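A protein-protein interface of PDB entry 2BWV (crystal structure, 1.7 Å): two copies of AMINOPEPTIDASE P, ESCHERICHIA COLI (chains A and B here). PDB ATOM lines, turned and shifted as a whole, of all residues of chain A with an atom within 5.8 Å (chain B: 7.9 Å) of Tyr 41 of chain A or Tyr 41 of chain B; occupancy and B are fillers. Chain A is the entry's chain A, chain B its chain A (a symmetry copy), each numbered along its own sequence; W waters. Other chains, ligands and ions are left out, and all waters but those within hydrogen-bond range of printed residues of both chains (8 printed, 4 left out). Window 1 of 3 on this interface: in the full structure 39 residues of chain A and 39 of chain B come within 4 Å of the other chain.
OH of Tyr 41 of chain B sits at hydrogen-bond distance from O of Pro 42 of chain A (2.7 Å).
O of Glu 40 of chain A sits at hydrogen-bond distance from ND2 of Asn 230 of chain B (2.9 Å).
NH1 of Arg 44 of chain A is in hydrogen-bond range of OG of Ser 36 of chain B, at 3.0 Å.
ND2 of Asn 230 of chain A lies within hydrogen-bond range of O of Glu 40 of chain B (2.9 Å).
The side-chain hydroxyl (OH) of Tyr 41 of chain A is in hydrogen-bond range of the backbone carbonyl oxygen (O) of Pro 42 of chain B, at 2.7 Å.
The backbone carbonyl oxygen (O) of Val 33 of chain B sits at hydrogen-bond distance from the backbone NH (N) of Tyr 41 of chain B (3.0 Å).
The backbone carbonyl oxygen of Ser 36 of chain B sits at hydrogen-bond distance from the side-chain hydroxyl of Ser 39 of chain B (2.8 Å).
The backbone carbonyl oxygen of Val 33 of chain A sits at hydrogen-bond distance from the backbone NH of Tyr 41 of chain A, at 3.0 Å.
OE2 of Glu 32 of chain B sits close to OE1 of Glu 40 of chain B, 2.6 Å away.
Arg 35 of chain A touches Arg 44 of chain B (O to CG, 3.5 Å).
Tyr 226 of chain B touches Arg 35 of chain A.
CD1 of Tyr 41 of chain A touches CD1 of Tyr 41 of chain B, at 3.4 Å.
Arg 44 of chain B touches Tyr 41 of chain A (N to OH, 3.5 Å).
Asn 230 of chain B touches Tyr 41 of chain A.
CG of Pro 42 of chain A touches OD1 of Asn 230 of chain B (3.4 Å).
Arg 44 of chain A touches Arg 35 of chain B (CG to O, 3.5 Å).
Tyr 41 of chain B touches Arg 44 of chain A (OH to N, 3.5 Å).
Tyr 41 of chain B touches Asn 230 of chain A (C to ND2, 3.7 Å).
Asn 230 of chain A touches Pro 42 of chain B (OD1 to CG, 3.4 Å).
Tyr 41 of chain A touches just these residues of chain B: Tyr 41 (3.4 Å), Pro 42 (2.7 Å), Arg 44 (3.5 Å) and Asn 230 (3.7 Å).
Of the printed residues of chain A, Tyr 41 of chain B touches Tyr 41 (3.4 Å), Pro 42 (2.7 Å), Arg 44 (3.5 Å) and Asn 230 (3.7 Å).
Of the printed residues of chain B, Asn 230 of chain A touches Glu 40 (2.9 Å), Tyr 41 (3.7 Å) and Pro 42 (3.4 Å).
Printed residues of chain B within 4 Å of Arg 44 of chain A: Arg 35, Ser 36 and Tyr 41.
Printed residues of chain A within 4 Å of Asn 230 of chain B: Glu 40 (2.9 Å), Tyr 41 (3.7 Å) and Pro 42 (3.4 Å).
Of the printed residues of chain B, Glu 40 of chain A touches Asn 230.
Of the printed residues of chain A, Val 33 of chain B touches Val 33 (2.8 Å).
Tyr 43 of chain A touches none of the printed residues of chain B.
The nearest printed residue of chain A that does not touch Glu 40 of chain B is Tyr 41 of chain A (7.1 Å).
Of the 19 printed residues of chain B, 9 touch a printed residue of chain A.
Printed residues of chain B that touch a printed residue of chain A: Val 33, Arg 35, Ser 36, Glu 40, Tyr 41, Pro 42, Arg 44, Tyr 226 and Asn 230.
Hydrophobic or aromatic side chains of chain B within 4 Å of the printed part of chain A: Val 33, Tyr 41, Pro 42 and Tyr 226.
Along chain B the printed residues that touch a printed residue of chain A span positions 33 to 230.
Printed residues of chain A that touch a printed residue of chain B: Val 33, Arg 35, Glu 40, Tyr 41, Pro 42, Arg 44 and Asn 230.
Hydrophobic or aromatic side chains of chain A within 4 Å of the printed part of chain B: Val 33, Tyr 41 and Pro 42.
Among the printed residues, no Asp or Glu carboxylate lies within 4 Å of a Lys or Arg side-chain nitrogen of the other chain.
Arg 35 of chain A touches Arg 44 of chain B, and with the chains exchanged Arg 44 of chain A touches Arg 35 of chain B.
Tyr 41 of chain B touches its own counterpart, Tyr 41 of chain A.
Tyr 41 of chain A touches Asn 230 of chain B, and with the chains exchanged Asn 230 of chain A touches Tyr 41 of chain B.
Pro 42 of chain A touches Asn 230 of chain B, and with the chains exchanged Asn 230 of chain A touches Pro 42 of chain B.
Positions printed for both chains: 33, 34, 35, 39, 40, 41, 42, 43, 44 and 230.
Of the 16 pairs that touch across the chains among the printed residues, 14 have their exchanged pair printed and touching as well.
Water W8 bridges OH of Tyr 41 of chain A (2.7 Å) and N of Arg 44 of chain B (3.1 Å).
Water W4 bridges the side-chain hydroxyl (OH) of Tyr 41 of chain B (2.7 Å) and the backbone NH (N) of Arg 44 of chain A (3.1 Å).
Water W1 bridges O of Tyr 43 of chain A (2.9 Å) and NH2 of Arg 35 of chain B (3.0 Å).
Water W3 bridges the backbone NH (N) of Asn 230 of chain B and the backbone carbonyl oxygen (O) of Glu 40 of chain A.
Water W2 bridges N of Asn 230 of chain A and O of Glu 40 of chain B.
Water W6 bridges OD1 of Asn 230 of chain B (3.1 Å) and O of Glu 40 of chain A (3.3 Å).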
ATOM      1  N   VAL A  33      24.363  16.230 -12.599  1.00  0.00           N
ATOM      2  CA  VAL A  33      23.950  14.832 -12.661  1.00  0.00           C
ATOM      3  C   VAL A  33      22.565  14.718 -13.331  1.00  0.00           C
ATOM      4  O   VAL A  33      21.613  15.344 -12.893  1.00  0.00           O
ATOM      5  CB  VAL A  33      23.840  14.273 -11.218  1.00  0.00           C
ATOM      6  CG1 VAL A  33      23.399  12.896 -11.233  1.00  0.00           C
ATOM      7  CG2 VAL A  33      25.160  14.346 -10.511  1.00  0.00           C
ATOM      8  N   THR A  34      22.468  13.897 -14.364  1.00  0.00           N
ATOM      9  CA  THR A  34      21.194  13.665 -15.052  1.00  0.00           C
ATOM     10  C   THR A  34      20.224  12.873 -14.168  1.00  0.00           C
ATOM     11  O   THR A  34      20.592  11.869 -13.558  1.00  0.00           O
ATOM     12  CB  THR A  34      21.419  12.892 -16.365  1.00  0.00           C
ATOM     13  OG1 THR A  34      22.164  13.709 -17.288  1.00  0.00           O
ATOM     14  CG2 THR A  34      20.091  12.462 -17.006  1.00  0.00           C
ATOM     15  N   ARG A  35      18.970  13.320 -14.129  1.00  0.00           N
ATOM     16  CA  ARG A  35      17.903  12.540 -13.541  1.00  0.00           C
ATOM     17  C   ARG A  35      17.205  11.721 -14.626  1.00  0.00           C
ATOM     18  O   ARG A  35      17.075  10.503 -14.502  1.00  0.00           O
ATOM     19  CB  ARG A  35      16.884  13.411 -12.792  1.00  0.00           C
ATOM     20  CG  ARG A  35      15.771  12.587 -12.204  1.00  0.00           C
ATOM     21  CD  ARG A  35      14.973  13.295 -11.101  1.00  0.00           C
ATOM     22  NE  ARG A  35      13.975  12.376 -10.526  1.00  0.00           N
ATOM     23  CZ  ARG A  35      12.776  12.098 -11.040  1.00  0.00           C
ATOM     24  NH1 ARG A  35      12.320  12.693 -12.134  1.00  0.00           N
ATOM     25  NH2 ARG A  35      11.998  11.212 -10.434  1.00  0.00           N
ATOM     26  N   SER A  39      16.556  16.549 -17.913  1.00  0.00           N
ATOM     27  CA  SER A  39      16.366  17.066 -16.563  1.00  0.00           C
ATOM     28  C   SER A  39      17.468  16.560 -15.635  1.00  0.00           C
ATOM     29  O   SER A  39      17.850  15.386 -15.699  1.00  0.00           O
ATOM     30  CB  SER A  39      14.994  16.691 -16.015  1.00  0.00           C
ATOM     31  OG  SER A  39      14.872  15.292 -15.818  1.00  0.00           O
ATOM     32  N   GLU A  40      17.976  17.454 -14.786  1.00  0.00           N
ATOM     33  CA  GLU A  40      19.017  17.120 -13.817  1.00  0.00           C
ATOM     34  C   GLU A  40      18.445  17.044 -12.409  1.00  0.00           C
ATOM     35  O   GLU A  40      17.420  17.672 -12.104  1.00  0.00           O
ATOM     36  CB  GLU A  40      20.126  18.172 -13.847  1.00  0.00           C
ATOM     37  CG  GLU A  40      20.818  18.290 -15.198  1.00  0.00           C
ATOM     38  CD  GLU A  40      21.590  19.591 -15.370  1.00  0.00           C
ATOM     39  OE1 GLU A  40      21.778  20.330 -14.376  1.00  0.00           O
ATOM     40  OE2 GLU A  40      22.002  19.871 -16.511  1.00  0.00           O
ATOM     41  N   TYR A  41      19.110  16.270 -11.563  1.00  0.00           N
ATOM     42  CA  TYR A  41      18.843  16.264 -10.139  1.00  0.00           C
ATOM     43  C   TYR A  41      19.249  17.643  -9.569  1.00  0.00           C
ATOM     44  O   TYR A  41      20.119  18.298 -10.128  1.00  0.00           O
ATOM     45  CB  TYR A  41      19.681  15.197  -9.448  1.00  0.00           C
ATOM     46  CG  TYR A  41      19.134  13.800  -9.542  1.00  0.00           C
ATOM     47  CD1 TYR A  41      18.061  13.393  -8.762  1.00  0.00           C
ATOM     48  CD2 TYR A  41      19.724  12.863 -10.396  1.00  0.00           C
ATOM     49  CE1 TYR A  41      17.560  12.098  -8.840  1.00  0.00           C
ATOM     50  CE2 TYR A  41      19.240  11.576 -10.487  1.00  0.00           C
ATOM     51  CZ  TYR A  41      18.164  11.184  -9.702  1.00  0.00           C
ATOM     52  OH  TYR A  41      17.692   9.895  -9.785  1.00  0.00           O
ATOM     53  N   PRO A  42      18.639  18.055  -8.449  1.00  0.00           N
ATOM     54  CA  PRO A  42      19.093  19.286  -7.774  1.00  0.00           C
ATOM     55  C   PRO A  42      20.583  19.154  -7.442  1.00  0.00           C
ATOM     56  O   PRO A  42      21.035  18.094  -6.978  1.00  0.00           O
ATOM     57  CB  PRO A  42      18.280  19.316  -6.474  1.00  0.00           C
ATOM     58  CG  PRO A  42      17.131  18.417  -6.700  1.00  0.00           C
ATOM     59  CD  PRO A  42      17.598  17.363  -7.677  1.00  0.00           C
ATOM     60  N   TYR A  43      21.327  20.208  -7.722  1.00  0.00           N
ATOM     61  CA  TYR A  43      22.782  20.163  -7.626  1.00  0.00           C
ATOM     62  C   TYR A  43      23.234  19.946  -6.186  1.00  0.00           C
ATOM     63  O   TYR A  43      22.717  20.580  -5.263  1.00  0.00           O
ATOM     64  CB  TYR A  43      23.413  21.449  -8.167  1.00  0.00           C
ATOM     65  CG  TYR A  43      24.914  21.390  -8.228  1.00  0.00           C
ATOM     66  CD1 TYR A  43      25.562  20.511  -9.094  1.00  0.00           C
ATOM     67  CD2 TYR A  43      25.710  22.206  -7.410  1.00  0.00           C
ATOM     68  CE1 TYR A  43      26.959  20.437  -9.134  1.00  0.00           C
ATOM     69  CE2 TYR A  43      27.088  22.153  -7.447  1.00  0.00           C
ATOM     70  CZ  TYR A  43      27.727  21.280  -8.318  1.00  0.00           C
ATOM     71  OH  TYR A  43      29.109  21.245  -8.351  1.00  0.00           O
ATOM     72  N   ARG A  44      24.178  19.029  -6.008  1.00  0.00           N
ATOM     73  CA  ARG A  44      24.846  18.845  -4.722  1.00  0.00           C
ATOM     74  C   ARG A  44      26.358  19.014  -4.917  1.00  0.00           C
ATOM     75  O   ARG A  44      27.012  18.219  -5.637  1.00  0.00           O
ATOM     76  CB  ARG A  44      24.514  17.462  -4.138  1.00  0.00           C
ATOM     77  CG  ARG A  44      25.362  17.108  -2.890  1.00  0.00           C
ATOM     78  CD  ARG A  44      25.324  18.182  -1.773  1.00  0.00           C
ATOM     79  NE  ARG A  44      25.418  17.501  -0.475  1.00  0.00           N
ATOM     80  CZ  ARG A  44      26.535  16.942   0.003  1.00  0.00           C
ATOM     81  NH1 ARG A  44      27.676  17.026  -0.666  1.00  0.00           N
ATOM     82  NH2 ARG A  44      26.519  16.291   1.172  1.00  0.00           N
ATOM     83  N   ASN A 230      18.493   9.440   1.613  1.00  0.00           N
ATOM     84  CA  ASN A 230      17.123   9.051   1.285  1.00  0.00           C
ATOM     85  C   ASN A 230      16.394   8.511   2.520  1.00  0.00           C
ATOM     86  O   ASN A 230      16.830   7.558   3.171  1.00  0.00           O
ATOM     87  CB  ASN A 230      17.119   8.039   0.151  1.00  0.00           C
ATOM     88  CG  ASN A 230      17.751   8.595  -1.112  1.00  0.00           C
ATOM     89  OD1 ASN A 230      17.614   9.781  -1.405  1.00  0.00           O
ATOM     90  ND2 ASN A 230      18.441   7.750  -1.850  1.00  0.00           N
ATOM     91  N   ALA B  30      18.531   2.530 -16.130  1.00  0.00           N
ATOM     92  CA  ALA B  30      19.389   3.627 -15.690  1.00  0.00           C
ATOM     93  C   ALA B  30      20.397   3.140 -14.640  1.00  0.00           C
ATOM     94  O   ALA B  30      20.084   2.270 -13.807  1.00  0.00           O
ATOM     95  CB  ALA B  30      18.567   4.783 -15.123  1.00  0.00           C
ATOM     96  N   PRO B  31      21.611   3.691 -14.683  1.00  0.00           N
ATOM     97  CA  PRO B  31      22.511   3.470 -13.550  1.00  0.00           C
ATOM     98  C   PRO B  31      22.026   4.219 -12.306  1.00  0.00           C
ATOM     99  O   PRO B  31      21.343   5.248 -12.412  1.00  0.00           O
ATOM    100  CB  PRO B  31      23.844   4.066 -14.018  1.00  0.00           C
ATOM    101  CG  PRO B  31      23.501   4.980 -15.135  1.00  0.00           C
ATOM    102  CD  PRO B  31      22.209   4.540 -15.729  1.00  0.00           C
ATOM    103  N   GLU B  32      22.364   3.688 -11.141  1.00  0.00           N
ATOM    104  CA  GLU B  32      22.297   4.466  -9.905  1.00  0.00           C
ATOM    105  C   GLU B  32      23.261   5.649 -10.007  1.00  0.00           C
ATOM    106  O   GLU B  32      24.269   5.581 -10.720  1.00  0.00           O
ATOM    107  CB  GLU B  32      22.641   3.580  -8.705  1.00  0.00           C
ATOM    108  CG  GLU B  32      21.622   2.483  -8.493  1.00  0.00           C
ATOM    109  CD  GLU B  32      21.805   1.707  -7.193  1.00  0.00           C
ATOM    110  OE1 GLU B  32      22.603   0.740  -7.168  1.00  0.00           O
ATOM    111  OE2 GLU B  32      21.108   2.050  -6.215  1.00  0.00           O
ATOM    112  N   VAL B  33      22.954   6.708  -9.267  1.00  0.00           N
ATOM    113  CA  VAL B  33      23.613   8.003  -9.394  1.00  0.00           C
ATOM    114  C   VAL B  33      24.062   8.506  -8.006  1.00  0.00           C
ATOM    115  O   VAL B  33      23.256   8.613  -7.097  1.00  0.00           O
ATOM    116  CB  VAL B  33      22.605   9.027  -9.980  1.00  0.00           C
ATOM    117  CG1 VAL B  33      23.210  10.336 -10.090  1.00  0.00           C
ATOM    118  CG2 VAL B  33      22.134   8.601 -11.338  1.00  0.00           C
ATOM    119  N   THR B  34      25.336   8.839  -7.877  1.00  0.00           N
ATOM    120  CA  THR B  34      25.873   9.377  -6.623  1.00  0.00           C
ATOM    121  C   THR B  34      25.346  10.792  -6.359  1.00  0.00           C
ATOM    122  O   THR B  34      25.339  11.646  -7.246  1.00  0.00           O
ATOM    123  CB  THR B  34      27.412   9.415  -6.663  1.00  0.00           C
ATOM    124  OG1 THR B  34      27.930   8.073  -6.709  1.00  0.00           O
ATOM    125  CG2 THR B  34      27.993  10.157  -5.449  1.00  0.00           C
ATOM    126  N   ARG B  35      24.931  11.039  -5.118  1.00  0.00           N
ATOM    127  CA  ARG B  35      24.643  12.384  -4.667  1.00  0.00           C
ATOM    128  C   ARG B  35      25.879  12.979  -3.996  1.00  0.00           C
ATOM    129  O   ARG B  35      26.330  14.062  -4.365  1.00  0.00           O
ATOM    130  CB  ARG B  35      23.441  12.437  -3.713  1.00  0.00           C
ATOM    131  CG  ARG B  35      23.166  13.839  -3.238  1.00  0.00           C
ATOM    132  CD  ARG B  35      21.764  14.047  -2.653  1.00  0.00           C
ATOM    133  NE  ARG B  35      21.562  15.465  -2.308  1.00  0.00           N
ATOM    134  CZ  ARG B  35      21.979  16.069  -1.194  1.00  0.00           C
ATOM    135  NH1 ARG B  35      22.588  15.410  -0.219  1.00  0.00           N
ATOM    136  NH2 ARG B  35      21.764  17.367  -1.040  1.00  0.00           N
ATOM    137  N   SER B  36      26.393  12.296  -2.966  1.00  0.00           N
ATOM    138  CA  SER B  36      27.666  12.667  -2.334  1.00  0.00           C
ATOM    139  C   SER B  36      28.293  11.442  -1.682  1.00  0.00           C
ATOM    140  O   SER B  36      27.642  10.748  -0.892  1.00  0.00           O
ATOM    141  CB  SER B  36      27.487  13.782  -1.302  1.00  0.00           C
ATOM    142  OG  SER B  36      28.692  14.153  -0.640  1.00  0.00           O
ATOM    143  N   ASP B  38      29.158   8.141  -0.457  1.00  0.00           N
ATOM    144  CA  ASP B  38      28.434   6.869  -0.506  1.00  0.00           C
ATOM    145  C   ASP B  38      26.908   6.997  -0.536  1.00  0.00           C
ATOM    146  O   ASP B  38      26.212   5.983  -0.521  1.00  0.00           O
ATOM    147  CB  ASP B  38      28.826   5.986   0.682  1.00  0.00           C
ATOM    148  CG  ASP B  38      30.289   5.618   0.678  1.00  0.00           C
ATOM    149  OD1 ASP B  38      30.808   5.236  -0.400  1.00  0.00           O
ATOM    150  OD2 ASP B  38      30.908   5.712   1.759  1.00  0.00           O
ATOM    151  N   SER B  39      26.371   8.216  -0.588  1.00  0.00           N
ATOM    152  CA  SER B  39      24.926   8.380  -0.683  1.00  0.00           C
ATOM    153  C   SER B  39      24.506   8.601  -2.135  1.00  0.00           C
ATOM    154  O   SER B  39      25.169   9.340  -2.872  1.00  0.00           O
ATOM    155  CB  SER B  39      24.440   9.528   0.192  1.00  0.00           C
ATOM    156  OG  SER B  39      24.914  10.781  -0.274  1.00  0.00           O
ATOM    157  N   GLU B  40      23.413   7.951  -2.536  1.00  0.00           N
ATOM    158  CA  GLU B  40      22.868   8.078  -3.885  1.00  0.00           C
ATOM    159  C   GLU B  40      21.602   8.920  -3.883  1.00  0.00           C
ATOM    160  O   GLU B  40      20.900   9.011  -2.864  1.00  0.00           O
ATOM    161  CB  GLU B  40      22.548   6.699  -4.459  1.00  0.00           C
ATOM    162  CG  GLU B  40      23.763   5.787  -4.570  1.00  0.00           C
ATOM    163  CD  GLU B  40      23.402   4.314  -4.714  1.00  0.00           C
ATOM    164  OE1 GLU B  40      22.212   3.992  -4.940  1.00  0.00           O
ATOM    165  OE2 GLU B  40      24.319   3.481  -4.593  1.00  0.00           O
ATOM    166  N   TYR B  41      21.321   9.534  -5.023  1.00  0.00           N
ATOM    167  CA  TYR B  41      20.048  10.181  -5.267  1.00  0.00           C
ATOM    168  C   TYR B  41      18.954   9.088  -5.309  1.00  0.00           C
ATOM    169  O   TYR B  41      19.250   7.948  -5.644  1.00  0.00           O
ATOM    170  CB  TYR B  41      20.064  10.893  -6.612  1.00  0.00           C
ATOM    171  CG  TYR B  41      20.732  12.239  -6.611  1.00  0.00           C
ATOM    172  CD1 TYR B  41      20.099  13.356  -6.083  1.00  0.00           C
ATOM    173  CD2 TYR B  41      21.998  12.404  -7.181  1.00  0.00           C
ATOM    174  CE1 TYR B  41      20.712  14.605  -6.091  1.00  0.00           C
ATOM    175  CE2 TYR B  41      22.619  13.633  -7.196  1.00  0.00           C
ATOM    176  CZ  TYR B  41      21.976  14.742  -6.661  1.00  0.00           C
ATOM    177  OH  TYR B  41      22.594  15.970  -6.690  1.00  0.00           O
ATOM    178  N   PRO B  42      17.701   9.452  -5.001  1.00  0.00           N
ATOM    179  CA  PRO B  42      16.594   8.493  -5.175  1.00  0.00           C
ATOM    180  C   PRO B  42      16.569   8.015  -6.630  1.00  0.00           C
ATOM    181  O   PRO B  42      16.727   8.821  -7.562  1.00  0.00           O
ATOM    182  CB  PRO B  42      15.337   9.324  -4.887  1.00  0.00           C
ATOM    183  CG  PRO B  42      15.803  10.508  -4.139  1.00  0.00           C
ATOM    184  CD  PRO B  42      17.215  10.779  -4.602  1.00  0.00           C
ATOM    185  N   TYR B  43      16.415   6.716  -6.803  1.00  0.00           N
ATOM    186  CA  TYR B  43      16.550   6.097  -8.118  1.00  0.00           C
ATOM    187  C   TYR B  43      15.460   6.581  -9.068  1.00  0.00           C
ATOM    188  O   TYR B  43      14.287   6.651  -8.695  1.00  0.00           O
ATOM    189  CB  TYR B  43      16.499   4.571  -8.021  1.00  0.00           C
ATOM    190  CG  TYR B  43      16.784   3.887  -9.330  1.00  0.00           C
ATOM    191  CD1 TYR B  43      18.041   3.973  -9.925  1.00  0.00           C
ATOM    192  CD2 TYR B  43      15.793   3.151  -9.999  1.00  0.00           C
ATOM    193  CE1 TYR B  43      18.300   3.357 -11.155  1.00  0.00           C
ATOM    194  CE2 TYR B  43      16.037   2.530 -11.206  1.00  0.00           C
ATOM    195  CZ  TYR B  43      17.295   2.613 -11.789  1.00  0.00           C
ATOM    196  OH  TYR B  43      17.528   1.976 -12.994  1.00  0.00           O
ATOM    197  N   ARG B  44      15.867   6.936 -10.283  1.00  0.00           N
ATOM    198  CA  ARG B  44      14.925   7.234 -11.358  1.00  0.00           C
ATOM    199  C   ARG B  44      15.219   6.313 -12.548  1.00  0.00           C
ATOM    200  O   ARG B  44      16.311   6.381 -13.167  1.00  0.00           O
ATOM    201  CB  ARG B  44      15.025   8.713 -11.764  1.00  0.00           C
ATOM    202  CG  ARG B  44      14.221   9.049 -13.046  1.00  0.00           C
ATOM    203  CD  ARG B  44      12.735   8.609 -12.994  1.00  0.00           C
ATOM    204  NE  ARG B  44      11.939   9.583 -13.754  1.00  0.00           N
ATOM    205  CZ  ARG B  44      11.938   9.677 -15.089  1.00  0.00           C
ATOM    206  NH1 ARG B  44      12.636   8.828 -15.829  1.00  0.00           N
ATOM    207  NH2 ARG B  44      11.227  10.631 -15.699  1.00  0.00           N
ATOM    208  N   GLN B  45      14.261   5.439 -12.852  1.00  0.00           N
ATOM    209  CA  GLN B  45      14.406   4.516 -13.966  1.00  0.00           C
ATOM    210  C   GLN B  45      14.446   5.300 -15.287  1.00  0.00           C
ATOM    211  O   GLN B  45      13.794   6.353 -15.412  1.00  0.00           O
ATOM    212  CB  GLN B  45      13.258   3.490 -13.983  1.00  0.00           C
ATOM    213  CG  GLN B  45      13.421   2.410 -15.034  1.00  0.00           C
ATOM    214  CD  GLN B  45      14.746   1.676 -14.897  1.00  0.00           C
ATOM    215  OE1 GLN B  45      15.749   2.063 -15.512  1.00  0.00           O
ATOM    216  NE2 GLN B  45      14.750   0.621 -14.087  1.00  0.00           N
ATOM    217  N   TYR B 226       7.917  12.279  -5.941  1.00  0.00           N
ATOM    218  CA  TYR B 226       8.945  13.178  -6.480  1.00  0.00           C
ATOM    219  C   TYR B 226       8.384  14.137  -7.529  1.00  0.00           C
ATOM    220  O   TYR B 226       7.495  13.747  -8.317  1.00  0.00           O
ATOM    221  CB  TYR B 226      10.083  12.388  -7.131  1.00  0.00           C
ATOM    222  CG  TYR B 226      10.673  11.346  -6.195  1.00  0.00           C
ATOM    223  CD1 TYR B 226      11.342  11.724  -5.039  1.00  0.00           C
ATOM    224  CD2 TYR B 226      10.515   9.992  -6.446  1.00  0.00           C
ATOM    225  CE1 TYR B 226      11.861  10.771  -4.157  1.00  0.00           C
ATOM    226  CE2 TYR B 226      11.024   9.041  -5.571  1.00  0.00           C
ATOM    227  CZ  TYR B 226      11.694   9.445  -4.432  1.00  0.00           C
ATOM    228  OH  TYR B 226      12.182   8.484  -3.570  1.00  0.00           O
ATOM    229  N   TYR B 229      10.539  17.627 -12.305  1.00  0.00           N
ATOM    230  CA  TYR B 229      11.671  18.507 -12.608  1.00  0.00           C
ATOM    231  C   TYR B 229      11.860  19.412 -11.399  1.00  0.00           C
ATOM    232  O   TYR B 229      10.990  19.488 -10.542  1.00  0.00           O
ATOM    233  CB  TYR B 229      11.435  19.350 -13.854  1.00  0.00           C
ATOM    234  CG  TYR B 229      10.145  20.118 -13.809  1.00  0.00           C
ATOM    235  CD1 TYR B 229       8.965  19.533 -14.245  1.00  0.00           C
ATOM    236  CD2 TYR B 229      10.087  21.430 -13.303  1.00  0.00           C
ATOM    237  CE1 TYR B 229       7.762  20.213 -14.187  1.00  0.00           C
ATOM    238  CE2 TYR B 229       8.873  22.136 -13.254  1.00  0.00           C
ATOM    239  CZ  TYR B 229       7.715  21.524 -13.704  1.00  0.00           C
ATOM    240  OH  TYR B 229       6.497  22.155 -13.685  1.00  0.00           O
ATOM    241  N   ASN B 230      12.993  20.087 -11.340  1.00  0.00           N
ATOM    242  CA  ASN B 230      13.277  20.929 -10.180  1.00  0.00           C
ATOM    243  C   ASN B 230      12.357  22.155 -10.151  1.00  0.00           C
ATOM    244  O   ASN B 230      12.300  22.950 -11.092  1.00  0.00           O
ATOM    245  CB  ASN B 230      14.741  21.333 -10.166  1.00  0.00           C
ATOM    246  CG  ASN B 230      15.664  20.129 -10.095  1.00  0.00           C
ATOM    247  OD1 ASN B 230      15.340  19.135  -9.449  1.00  0.00           O
ATOM    248  ND2 ASN B 230      16.799  20.215 -10.757  1.00  0.00           N
ATOM    249  N   THR B 245      15.953  28.074  -9.948  1.00  0.00           N
ATOM    250  CA  THR B 245      15.631  27.023  -8.970  1.00  0.00           C
ATOM    251  C   THR B 245      16.285  27.241  -7.600  1.00  0.00           C
ATOM    252  O   THR B 245      16.093  26.417  -6.702  1.00  0.00           O
ATOM    253  CB  THR B 245      16.036  25.625  -9.504  1.00  0.00           C
ATOM    254  OG1 THR B 245      17.452  25.607  -9.730  1.00  0.00           O
ATOM    255  CG2 THR B 245      15.269  25.276 -10.794  1.00  0.00           C
HETATM  256  O   HOH W   1      21.184  19.252  -3.255  1.00  0.00           O
HETATM  257  O   HOH W   2      20.855   8.602   0.120  1.00  0.00           O
HETATM  258  O   HOH W   3      15.009  19.103 -13.205  1.00  0.00           O
HETATM  259  O   HOH W   4      24.379  17.113  -8.387  1.00  0.00           O
HETATM  260  O   HOH W   5      20.095  11.582  -0.954  1.00  0.00           O
HETATM  261  O   HOH W   6      14.432  16.680 -11.105  1.00  0.00           O
HETATM  262  O   HOH W   7      12.959   9.170  -8.510  1.00  0.00           O
HETATM  263  O   HOH W   8      18.871   7.518 -10.361  1.00  0.00           O
